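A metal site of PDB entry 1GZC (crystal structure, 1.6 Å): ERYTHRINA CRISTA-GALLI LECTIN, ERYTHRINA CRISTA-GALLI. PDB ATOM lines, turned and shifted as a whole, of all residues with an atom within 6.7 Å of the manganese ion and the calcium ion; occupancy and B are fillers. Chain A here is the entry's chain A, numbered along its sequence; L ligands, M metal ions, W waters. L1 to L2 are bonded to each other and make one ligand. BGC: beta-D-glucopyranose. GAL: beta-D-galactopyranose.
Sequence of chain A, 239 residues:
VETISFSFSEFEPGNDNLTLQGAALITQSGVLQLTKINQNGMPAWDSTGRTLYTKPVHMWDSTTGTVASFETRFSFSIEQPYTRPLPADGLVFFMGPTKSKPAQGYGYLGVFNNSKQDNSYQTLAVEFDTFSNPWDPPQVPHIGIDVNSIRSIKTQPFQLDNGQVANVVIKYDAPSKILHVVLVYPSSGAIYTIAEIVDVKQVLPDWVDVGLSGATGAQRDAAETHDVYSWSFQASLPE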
ATOM      1  N   ASP A  89      -3.692  -6.288   9.734  1.00  0.00           N
ATOM      2  CA  ASP A  89      -3.921  -7.114  10.925  1.00  0.00           C
ATOM      3  C   ASP A  89      -5.155  -8.014  10.731  1.00  0.00           C
ATOM      4  O   ASP A  89      -5.248  -9.034  11.383  1.00  0.00           O
ATOM      5  CB  ASP A  89      -4.156  -6.225  12.136  1.00  0.00           C
ATOM      6  CG  ASP A  89      -2.861  -5.942  12.929  1.00  0.00           C
ATOM      7  OD1 ASP A  89      -2.380  -6.906  13.603  1.00  0.00           O
ATOM      8  OD2 ASP A  89      -2.335  -4.779  12.869  1.00  0.00           O
ATOM      9  N   TYR A 106      -4.736  -1.955  15.151  1.00  0.00           N
ATOM     10  CA  TYR A 106      -3.741  -3.034  15.029  1.00  0.00           C
ATOM     11  C   TYR A 106      -4.391  -4.387  15.342  1.00  0.00           C
ATOM     12  O   TYR A 106      -5.458  -4.691  14.791  1.00  0.00           O
ATOM     13  CB  TYR A 106      -2.510  -2.763  15.930  1.00  0.00           C
ATOM     14  CG  TYR A 106      -1.902  -1.389  15.690  1.00  0.00           C
ATOM     15  CD1 TYR A 106      -1.824  -0.852  14.416  1.00  0.00           C
ATOM     16  CD2 TYR A 106      -1.404  -0.620  16.764  1.00  0.00           C
ATOM     17  CE1 TYR A 106      -1.259   0.430  14.194  1.00  0.00           C
ATOM     18  CE2 TYR A 106      -0.856   0.649  16.565  1.00  0.00           C
ATOM     19  CZ  TYR A 106      -0.792   1.160  15.283  1.00  0.00           C
ATOM     20  OH  TYR A 106      -0.275   2.429  15.105  1.00  0.00           O
ATOM     21  N   GLY A 107      -3.771  -5.199  16.213  1.00  0.00           N
ATOM     22  CA  GLY A 107      -4.327  -6.510  16.499  1.00  0.00           C
ATOM     23  C   GLY A 107      -5.670  -6.536  17.206  1.00  0.00           C
ATOM     24  O   GLY A 107      -6.287  -7.616  17.323  1.00  0.00           O
ATOM     25  N   TYR A 108      -6.139  -5.379  17.696  1.00  0.00           N
ATOM     26  CA  TYR A 108      -7.448  -5.310  18.354  1.00  0.00           C
ATOM     27  C   TYR A 108      -8.576  -5.095  17.342  1.00  0.00           C
ATOM     28  O   TYR A 108      -9.763  -5.097  17.723  1.00  0.00           O
ATOM     29  CB  TYR A 108      -7.444  -4.229  19.439  1.00  0.00           C
ATOM     30  CG  TYR A 108      -6.339  -4.493  20.444  1.00  0.00           C
ATOM     31  CD1 TYR A 108      -6.330  -5.645  21.189  1.00  0.00           C
ATOM     32  CD2 TYR A 108      -5.298  -3.592  20.616  1.00  0.00           C
ATOM     33  CE1 TYR A 108      -5.290  -5.931  22.114  1.00  0.00           C
ATOM     34  CE2 TYR A 108      -4.248  -3.869  21.545  1.00  0.00           C
ATOM     35  CZ  TYR A 108      -4.272  -5.039  22.264  1.00  0.00           C
ATOM     36  OH  TYR A 108      -3.239  -5.374  23.141  1.00  0.00           O
ATOM     37  N   LEU A 109      -8.172  -4.924  16.069  1.00  0.00           N
ATOM     38  CA  LEU A 109      -9.057  -4.893  14.883  1.00  0.00           C
ATOM     39  C   LEU A 109     -10.177  -3.851  14.905  1.00  0.00           C
ATOM     40  O   LEU A 109     -11.181  -4.000  14.227  1.00  0.00           O
ATOM     41  CB  LEU A 109      -9.725  -6.280  14.696  1.00  0.00           C
ATOM     42  CG  LEU A 109      -8.670  -7.397  14.613  1.00  0.00           C
ATOM     43  CD1 LEU A 109      -9.390  -8.758  14.513  1.00  0.00           C
ATOM     44  CD2 LEU A 109      -7.721  -7.206  13.385  1.00  0.00           C
ATOM     45  N   GLU A 127     -13.608 -13.131  13.654  1.00  0.00           N
ATOM     46  CA  GLU A 127     -12.461 -12.486  12.994  1.00  0.00           C
ATOM     47  C   GLU A 127     -11.792 -13.314  11.910  1.00  0.00           C
ATOM     48  O   GLU A 127     -11.870 -14.551  11.928  1.00  0.00           O
ATOM     49  CB  GLU A 127     -11.431 -12.180  14.078  1.00  0.00           C
ATOM     50  CG  GLU A 127     -10.898 -13.471  14.768  1.00  0.00           C
ATOM     51  CD  GLU A 127      -9.671 -13.203  15.660  1.00  0.00           C
ATOM     52  OE1 GLU A 127      -9.749 -12.292  16.501  1.00  0.00           O
ATOM     53  OE2 GLU A 127      -8.648 -13.950  15.514  1.00  0.00           O
ATOM     54  N   ASP A 129      -8.159 -13.103  10.887  1.00  0.00           N
ATOM     55  CA  ASP A 129      -6.945 -12.492  11.448  1.00  0.00           C
ATOM     56  C   ASP A 129      -5.692 -12.884  10.698  1.00  0.00           C
ATOM     57  O   ASP A 129      -5.393 -14.077  10.542  1.00  0.00           O
ATOM     58  CB  ASP A 129      -6.869 -13.001  12.894  1.00  0.00           C
ATOM     59  CG  ASP A 129      -5.781 -12.336  13.750  1.00  0.00           C
ATOM     60  OD1 ASP A 129      -4.950 -11.629  13.225  1.00  0.00           O
ATOM     61  OD2 ASP A 129      -5.807 -12.534  15.000  1.00  0.00           O
ATOM     62  N   THR A 130      -4.946 -11.871  10.255  1.00  0.00           N
ATOM     63  CA  THR A 130      -3.784 -12.109   9.432  1.00  0.00           C
ATOM     64  C   THR A 130      -2.419 -11.934  10.085  1.00  0.00           C
ATOM     65  O   THR A 130      -1.400 -12.195   9.413  1.00  0.00           O
ATOM     66  CB  THR A 130      -3.868 -11.188   8.226  1.00  0.00           C
ATOM     67  OG1 THR A 130      -3.976  -9.843   8.719  1.00  0.00           O
ATOM     68  CG2 THR A 130      -5.160 -11.510   7.390  1.00  0.00           C
ATOM     69  N   PHE A 131      -2.372 -11.555  11.357  1.00  0.00           N
ATOM     70  CA  PHE A 131      -1.094 -11.349  12.029  1.00  0.00           C
ATOM     71  C   PHE A 131      -1.116 -12.061  13.362  1.00  0.00           C
ATOM     72  O   PHE A 131      -2.054 -11.881  14.137  1.00  0.00           O
ATOM     73  CB  PHE A 131      -0.837  -9.831  12.233  1.00  0.00           C
ATOM     74  CG  PHE A 131       0.498  -9.549  12.889  1.00  0.00           C
ATOM     75  CD1 PHE A 131       1.663  -9.392  12.105  1.00  0.00           C
ATOM     76  CD2 PHE A 131       0.586  -9.528  14.273  1.00  0.00           C
ATOM     77  CE1 PHE A 131       2.925  -9.217  12.738  1.00  0.00           C
ATOM     78  CE2 PHE A 131       1.818  -9.352  14.928  1.00  0.00           C
ATOM     79  CZ  PHE A 131       2.989  -9.203  14.145  1.00  0.00           C
ATOM     80  N   SER A 132      -0.078 -12.875  13.631  1.00  0.00           N
ATOM     81  CA  SER A 132      -0.042 -13.606  14.894  1.00  0.00           C
ATOM     82  C   SER A 132       0.531 -12.764  16.059  1.00  0.00           C
ATOM     83  O   SER A 132       1.765 -12.605  16.200  1.00  0.00           O
ATOM     84  CB  SER A 132       0.783 -14.905  14.748  1.00  0.00           C
ATOM     85  OG  SER A 132       0.615 -15.691  15.925  1.00  0.00           O
ATOM     86  N   ASN A 133      -0.354 -12.186  16.866  1.00  0.00           N
ATOM     87  CA  ASN A 133      -0.011 -11.401  18.034  1.00  0.00           C
ATOM     88  C   ASN A 133       0.353 -12.355  19.220  1.00  0.00           C
ATOM     89  O   ASN A 133       0.217 -13.597  19.126  1.00  0.00           O
ATOM     90  CB  ASN A 133      -1.215 -10.518  18.430  1.00  0.00           C
ATOM     91  CG  ASN A 133      -1.522  -9.490  17.399  1.00  0.00           C
ATOM     92  OD1 ASN A 133      -2.369  -9.687  16.501  1.00  0.00           O
ATOM     93  ND2 ASN A 133      -0.809  -8.365  17.478  1.00  0.00           N
ATOM     94  N   TRP A 135      -1.193 -13.081  21.851  1.00  0.00           N
ATOM     95  CA  TRP A 135      -2.335 -13.872  22.294  1.00  0.00           C
ATOM     96  C   TRP A 135      -2.926 -14.804  21.227  1.00  0.00           C
ATOM     97  O   TRP A 135      -3.895 -15.478  21.483  1.00  0.00           O
ATOM     98  CB  TRP A 135      -3.463 -12.917  22.737  1.00  0.00           C
ATOM     99  CG  TRP A 135      -3.858 -11.947  21.613  1.00  0.00           C
ATOM    100  CD1 TRP A 135      -4.702 -12.207  20.535  1.00  0.00           C
ATOM    101  CD2 TRP A 135      -3.377 -10.603  21.431  1.00  0.00           C
ATOM    102  NE1 TRP A 135      -4.749 -11.095  19.705  1.00  0.00           N
ATOM    103  CE2 TRP A 135      -3.962 -10.102  20.227  1.00  0.00           C
ATOM    104  CE3 TRP A 135      -2.517  -9.773  22.159  1.00  0.00           C
ATOM    105  CZ2 TRP A 135      -3.702  -8.813  19.762  1.00  0.00           C
ATOM    106  CZ3 TRP A 135      -2.254  -8.495  21.685  1.00  0.00           C
ATOM    107  CH2 TRP A 135      -2.855  -8.023  20.487  1.00  0.00           C
ATOM    108  N   ASP A 136      -2.332 -14.846  20.057  1.00  0.00           N
ATOM    109  CA  ASP A 136      -2.871 -15.630  18.926  1.00  0.00           C
ATOM    110  C   ASP A 136      -2.201 -16.978  18.708  1.00  0.00           C
ATOM    111  O   ASP A 136      -1.087 -17.201  19.174  1.00  0.00           O
ATOM    112  CB  ASP A 136      -2.580 -14.878  17.605  1.00  0.00           C
ATOM    113  CG  ASP A 136      -3.593 -13.791  17.278  1.00  0.00           C
ATOM    114  OD1 ASP A 136      -4.784 -14.034  17.505  1.00  0.00           O
ATOM    115  OD2 ASP A 136      -3.190 -12.725  16.768  1.00  0.00           O
ATOM    116  N   PRO A 137      -2.889 -17.882  17.969  1.00  0.00           N
ATOM    117  CA  PRO A 137      -2.283 -19.175  17.640  1.00  0.00           C
ATOM    118  C   PRO A 137      -1.276 -18.721  16.562  1.00  0.00           C
ATOM    119  O   PRO A 137      -1.386 -17.619  16.018  1.00  0.00           O
ATOM    120  CB  PRO A 137      -3.460 -19.970  17.034  1.00  0.00           C
ATOM    121  CG  PRO A 137      -4.395 -18.828  16.478  1.00  0.00           C
ATOM    122  CD  PRO A 137      -4.319 -17.827  17.613  1.00  0.00           C
ATOM    123  N   VAL A 140      -1.440 -18.139  10.633  1.00  0.00           N
ATOM    124  CA  VAL A 140      -2.189 -17.019  10.063  1.00  0.00           C
ATOM    125  C   VAL A 140      -2.231 -17.210   8.535  1.00  0.00           C
ATOM    126  O   VAL A 140      -1.289 -17.672   7.890  1.00  0.00           O
ATOM    127  CB  VAL A 140      -1.604 -15.643  10.396  1.00  0.00           C
ATOM    128  CG1 VAL A 140      -1.957 -15.260  11.845  1.00  0.00           C
ATOM    129  CG2 VAL A 140      -0.063 -15.621  10.209  1.00  0.00           C
ATOM    130  N   HIS A 142      -6.203 -16.953  10.268  1.00  0.00           N
ATOM    131  CA  HIS A 142      -7.087 -17.858  10.967  1.00  0.00           C
ATOM    132  C   HIS A 142      -8.461 -17.219  11.180  1.00  0.00           C
ATOM    133  O   HIS A 142      -8.586 -16.007  11.311  1.00  0.00           O
ATOM    134  CB  HIS A 142      -6.536 -18.323  12.361  1.00  0.00           C
ATOM    135  CG  HIS A 142      -6.143 -17.211  13.318  1.00  0.00           C
ATOM    136  ND1 HIS A 142      -4.848 -16.744  13.453  1.00  0.00           N
ATOM    137  CD2 HIS A 142      -6.892 -16.508  14.197  1.00  0.00           C
ATOM    138  CE1 HIS A 142      -4.821 -15.788  14.375  1.00  0.00           C
ATOM    139  NE2 HIS A 142      -6.050 -15.620  14.841  1.00  0.00           N
ATOM    140  N   ILE A 143      -9.489 -18.068  11.220  1.00  0.00           N
ATOM    141  CA  ILE A 143     -10.832 -17.605  11.603  1.00  0.00           C
ATOM    142  C   ILE A 143     -10.827 -17.717  13.113  1.00  0.00           C
ATOM    143  O   ILE A 143     -10.248 -18.680  13.672  1.00  0.00           O
ATOM    144  CB  ILE A 143     -11.930 -18.554  11.051  1.00  0.00           C
ATOM    145  CG1 ILE A 143     -11.762 -18.691   9.529  1.00  0.00           C
ATOM    146  CG2 ILE A 143     -13.301 -17.951  11.287  1.00  0.00           C
ATOM    147  CD1 ILE A 143     -12.798 -19.629   8.929  1.00  0.00           C
ATOM    148  N   GLY A 144     -11.466 -16.767  13.789  1.00  0.00           N
ATOM    149  CA  GLY A 144     -11.559 -16.836  15.251  1.00  0.00           C
ATOM    150  C   GLY A 144     -12.945 -16.456  15.771  1.00  0.00           C
ATOM    151  O   GLY A 144     -13.611 -15.556  15.223  1.00  0.00           O
ATOM    152  N   ASP A 146     -14.605 -14.825  18.845  1.00  0.00           N
ATOM    153  CA  ASP A 146     -14.208 -13.929  19.951  1.00  0.00           C
ATOM    154  C   ASP A 146     -15.403 -13.572  20.807  1.00  0.00           C
ATOM    155  O   ASP A 146     -16.368 -12.933  20.342  1.00  0.00           O
ATOM    156  CB  ASP A 146     -13.639 -12.627  19.370  1.00  0.00           C
ATOM    157  CG  ASP A 146     -12.416 -12.841  18.471  1.00  0.00           C
ATOM    158  OD1 ASP A 146     -11.895 -13.978  18.406  1.00  0.00           O
ATOM    159  OD2 ASP A 146     -11.960 -11.844  17.845  1.00  0.00           O
ATOM    160  N   ILE A 150     -10.315 -10.394  22.493  1.00  0.00           N
ATOM    161  CA  ILE A 150      -9.588 -10.579  21.230  1.00  0.00           C
ATOM    162  C   ILE A 150      -8.870 -11.974  21.284  1.00  0.00           C
ATOM    163  O   ILE A 150      -8.401 -12.455  20.251  1.00  0.00           O
ATOM    164  CB  ILE A 150      -8.550  -9.437  21.028  1.00  0.00           C
ATOM    165  CG1 ILE A 150      -7.967  -9.464  19.621  1.00  0.00           C
ATOM    166  CG2 ILE A 150      -7.338  -9.660  22.002  1.00  0.00           C
ATOM    167  CD1 ILE A 150      -9.033  -9.200  18.500  1.00  0.00           C
ATOM    168  N   ARG A 151      -8.789 -12.604  22.458  1.00  0.00           N
ATOM    169  CA  ARG A 151      -8.141 -13.939  22.549  1.00  0.00           C
ATOM    170  C   ARG A 151      -9.281 -14.947  22.295  1.00  0.00           C
ATOM    171  O   ARG A 151     -10.084 -15.284  23.187  1.00  0.00           O
ATOM    172  CB  ARG A 151      -7.561 -14.161  23.963  1.00  0.00           C
ATOM    173  CG  ARG A 151      -6.617 -13.064  24.366  1.00  0.00           C
ATOM    174  CD  ARG A 151      -5.766 -13.514  25.590  1.00  0.00           C
ATOM    175  NE  ARG A 151      -4.856 -12.446  25.994  1.00  0.00           N
ATOM    176  CZ  ARG A 151      -3.579 -12.627  26.317  1.00  0.00           C
ATOM    177  NH1 ARG A 151      -3.073 -13.854  26.292  1.00  0.00           N
ATOM    178  NH2 ARG A 151      -2.806 -11.572  26.549  1.00  0.00           N
ATOM    179  N   SER A 152      -9.328 -15.419  21.058  1.00  0.00           N
ATOM    180  CA  SER A 152     -10.435 -16.287  20.637  1.00  0.00           C
ATOM    181  C   SER A 152     -10.611 -17.531  21.473  1.00  0.00           C
ATOM    182  O   SER A 152      -9.629 -18.158  21.871  1.00  0.00           O
ATOM    183  CB  SER A 152     -10.228 -16.774  19.191  1.00  0.00           C
ATOM    184  OG  SER A 152      -9.891 -15.712  18.299  1.00  0.00           O
ATOM    185  N   THR A 155     -10.202 -21.174  17.215  1.00  0.00           N
ATOM    186  CA  THR A 155      -9.727 -20.700  15.925  1.00  0.00           C
ATOM    187  C   THR A 155      -9.603 -21.836  14.916  1.00  0.00           C
ATOM    188  O   THR A 155      -9.547 -23.024  15.275  1.00  0.00           O
ATOM    189  CB  THR A 155      -8.355 -20.018  16.029  1.00  0.00           C
ATOM    190  OG1 THR A 155      -7.369 -20.955  16.567  1.00  0.00           O
ATOM    191  CG2 THR A 155      -8.461 -18.831  16.954  1.00  0.00           C
HETATM  192  C2  BGC L   1       6.863  -2.518  16.045  1.00  0.00           C
HETATM  193  C3  BGC L   1       5.330  -2.627  15.812  1.00  0.00           C
HETATM  194  C4  BGC L   1       4.711  -3.640  16.786  1.00  0.00           C
HETATM  195  C5  BGC L   1       5.044  -3.301  18.253  1.00  0.00           C
HETATM  196  C6  BGC L   1       4.586  -4.413  19.208  1.00  0.00           C
HETATM  197  C1  BGC L   1       7.079  -2.136  17.504  1.00  0.00           C
HETATM  198  O1  BGC L   1       8.452  -2.035  17.753  1.00  0.00           O
HETATM  199  O2  BGC L   1       7.373  -1.543  15.148  1.00  0.00           O
HETATM  200  O3  BGC L   1       5.101  -2.987  14.451  1.00  0.00           O
HETATM  201  O4  BGC L   1       3.229  -3.667  16.706  1.00  0.00           O
HETATM  202  O5  BGC L   1       6.516  -3.188  18.360  1.00  0.00           O
HETATM  203  O6  BGC L   1       4.835  -4.050  20.561  1.00  0.00           O
HETATM  204  C1  GAL L   2       2.628  -4.761  15.987  1.00  0.00           C
HETATM  205  C2  GAL L   2       1.129  -4.806  16.270  1.00  0.00           C
HETATM  206  C3  GAL L   2       0.534  -5.997  15.417  1.00  0.00           C
HETATM  207  C4  GAL L   2       0.855  -5.739  13.937  1.00  0.00           C
HETATM  208  C5  GAL L   2       2.372  -5.618  13.753  1.00  0.00           C
HETATM  209  C6  GAL L   2       2.762  -5.282  12.320  1.00  0.00           C
HETATM  210  O2  GAL L   2       0.867  -5.003  17.672  1.00  0.00           O
HETATM  211  O3  GAL L   2      -0.867  -6.092  15.651  1.00  0.00           O
HETATM  212  O4  GAL L   2       0.304  -4.517  13.460  1.00  0.00           O
HETATM  213  O5  GAL L   2       2.894  -4.560  14.594  1.00  0.00           O
HETATM  214  O6  GAL L   2       4.174  -5.492  12.200  1.00  0.00           O
HETATM  215 MN    MN M   1      -6.640 -13.995  16.359  1.00  0.00          MN
HETATM  216 CA    CA M   2      -3.905 -11.001  15.332  1.00  0.00          CA
HETATM  217  O   HOH W   1      -7.355 -12.270  17.601  1.00  0.00           O
HETATM  218  O   HOH W   2      -7.281 -15.507  17.804  1.00  0.00           O
HETATM  219  O   HOH W   3      -5.586 -10.149  16.850  1.00  0.00           O
HETATM  220  O   HOH W   4      -3.945  -9.045  13.960  1.00  0.00           O
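Water W1 bridges OE1 of Glu 127 (2.6 Å) and O of Ile 150 (2.9 Å).
Water W3 lies within hydrogen-bond range of the backbone carbonyl oxygen (O) of Gly 107 (2.7 Å) and the indole nitrogen (NE1) of Trp 135 (3.1 Å).
Four residues have an atom within 4 Å of the calcium ion: Asp 129, Phe 131, Asn 133 and Asp 136.
The manganese ion is bound by OD2 of Asp 129 (2.2 Å), OE2 of Glu 127 (2.2 Å), OD1 of Asp 136 (2.2 Å), water W2 (2.2 Å), water W1 (2.2 Å) and NE2 of His 142 (2.3 Å).
The manganese ion has six donor atoms within binding distance.
OE1 of Glu 127 lies close to OD2 of Asp 146.
The backbone NH (N) of Glu 127 lies within hydrogen-bond range of the backbone carbonyl oxygen (O) of Gly 144 (2.9 Å).
The calcium ion is bound by the side-chain amide oxygen (OD1) of Asn 133 (2.3 Å), the side-chain carboxylate (OD2) of Asp 136 (2.4 Å), the backbone carbonyl oxygen (O) of Phe 131 (2.4 Å), water W4 (2.4 Å), water W3 (2.4 Å), the side-chain carboxylate (OD1) of Asp 129 (2.4 Å) and the side-chain carboxylate (OD2) of Asp 129 (2.5 Å).
The calcium ion has seven donor atoms within binding distance.
Within 4 Å of the manganese ion: Glu 127, Asp 129, Asp 136 and His 142.
ND2 of Asn 133 sits at hydrogen-bond distance from O3 of GAL L2 (2.9 Å).
N of Gly 107 sits at hydrogen-bond distance from O3 of GAL L2.
OD1 of Asp 89 is in hydrogen-bond range of O3 of GAL L2 (2.7 Å).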
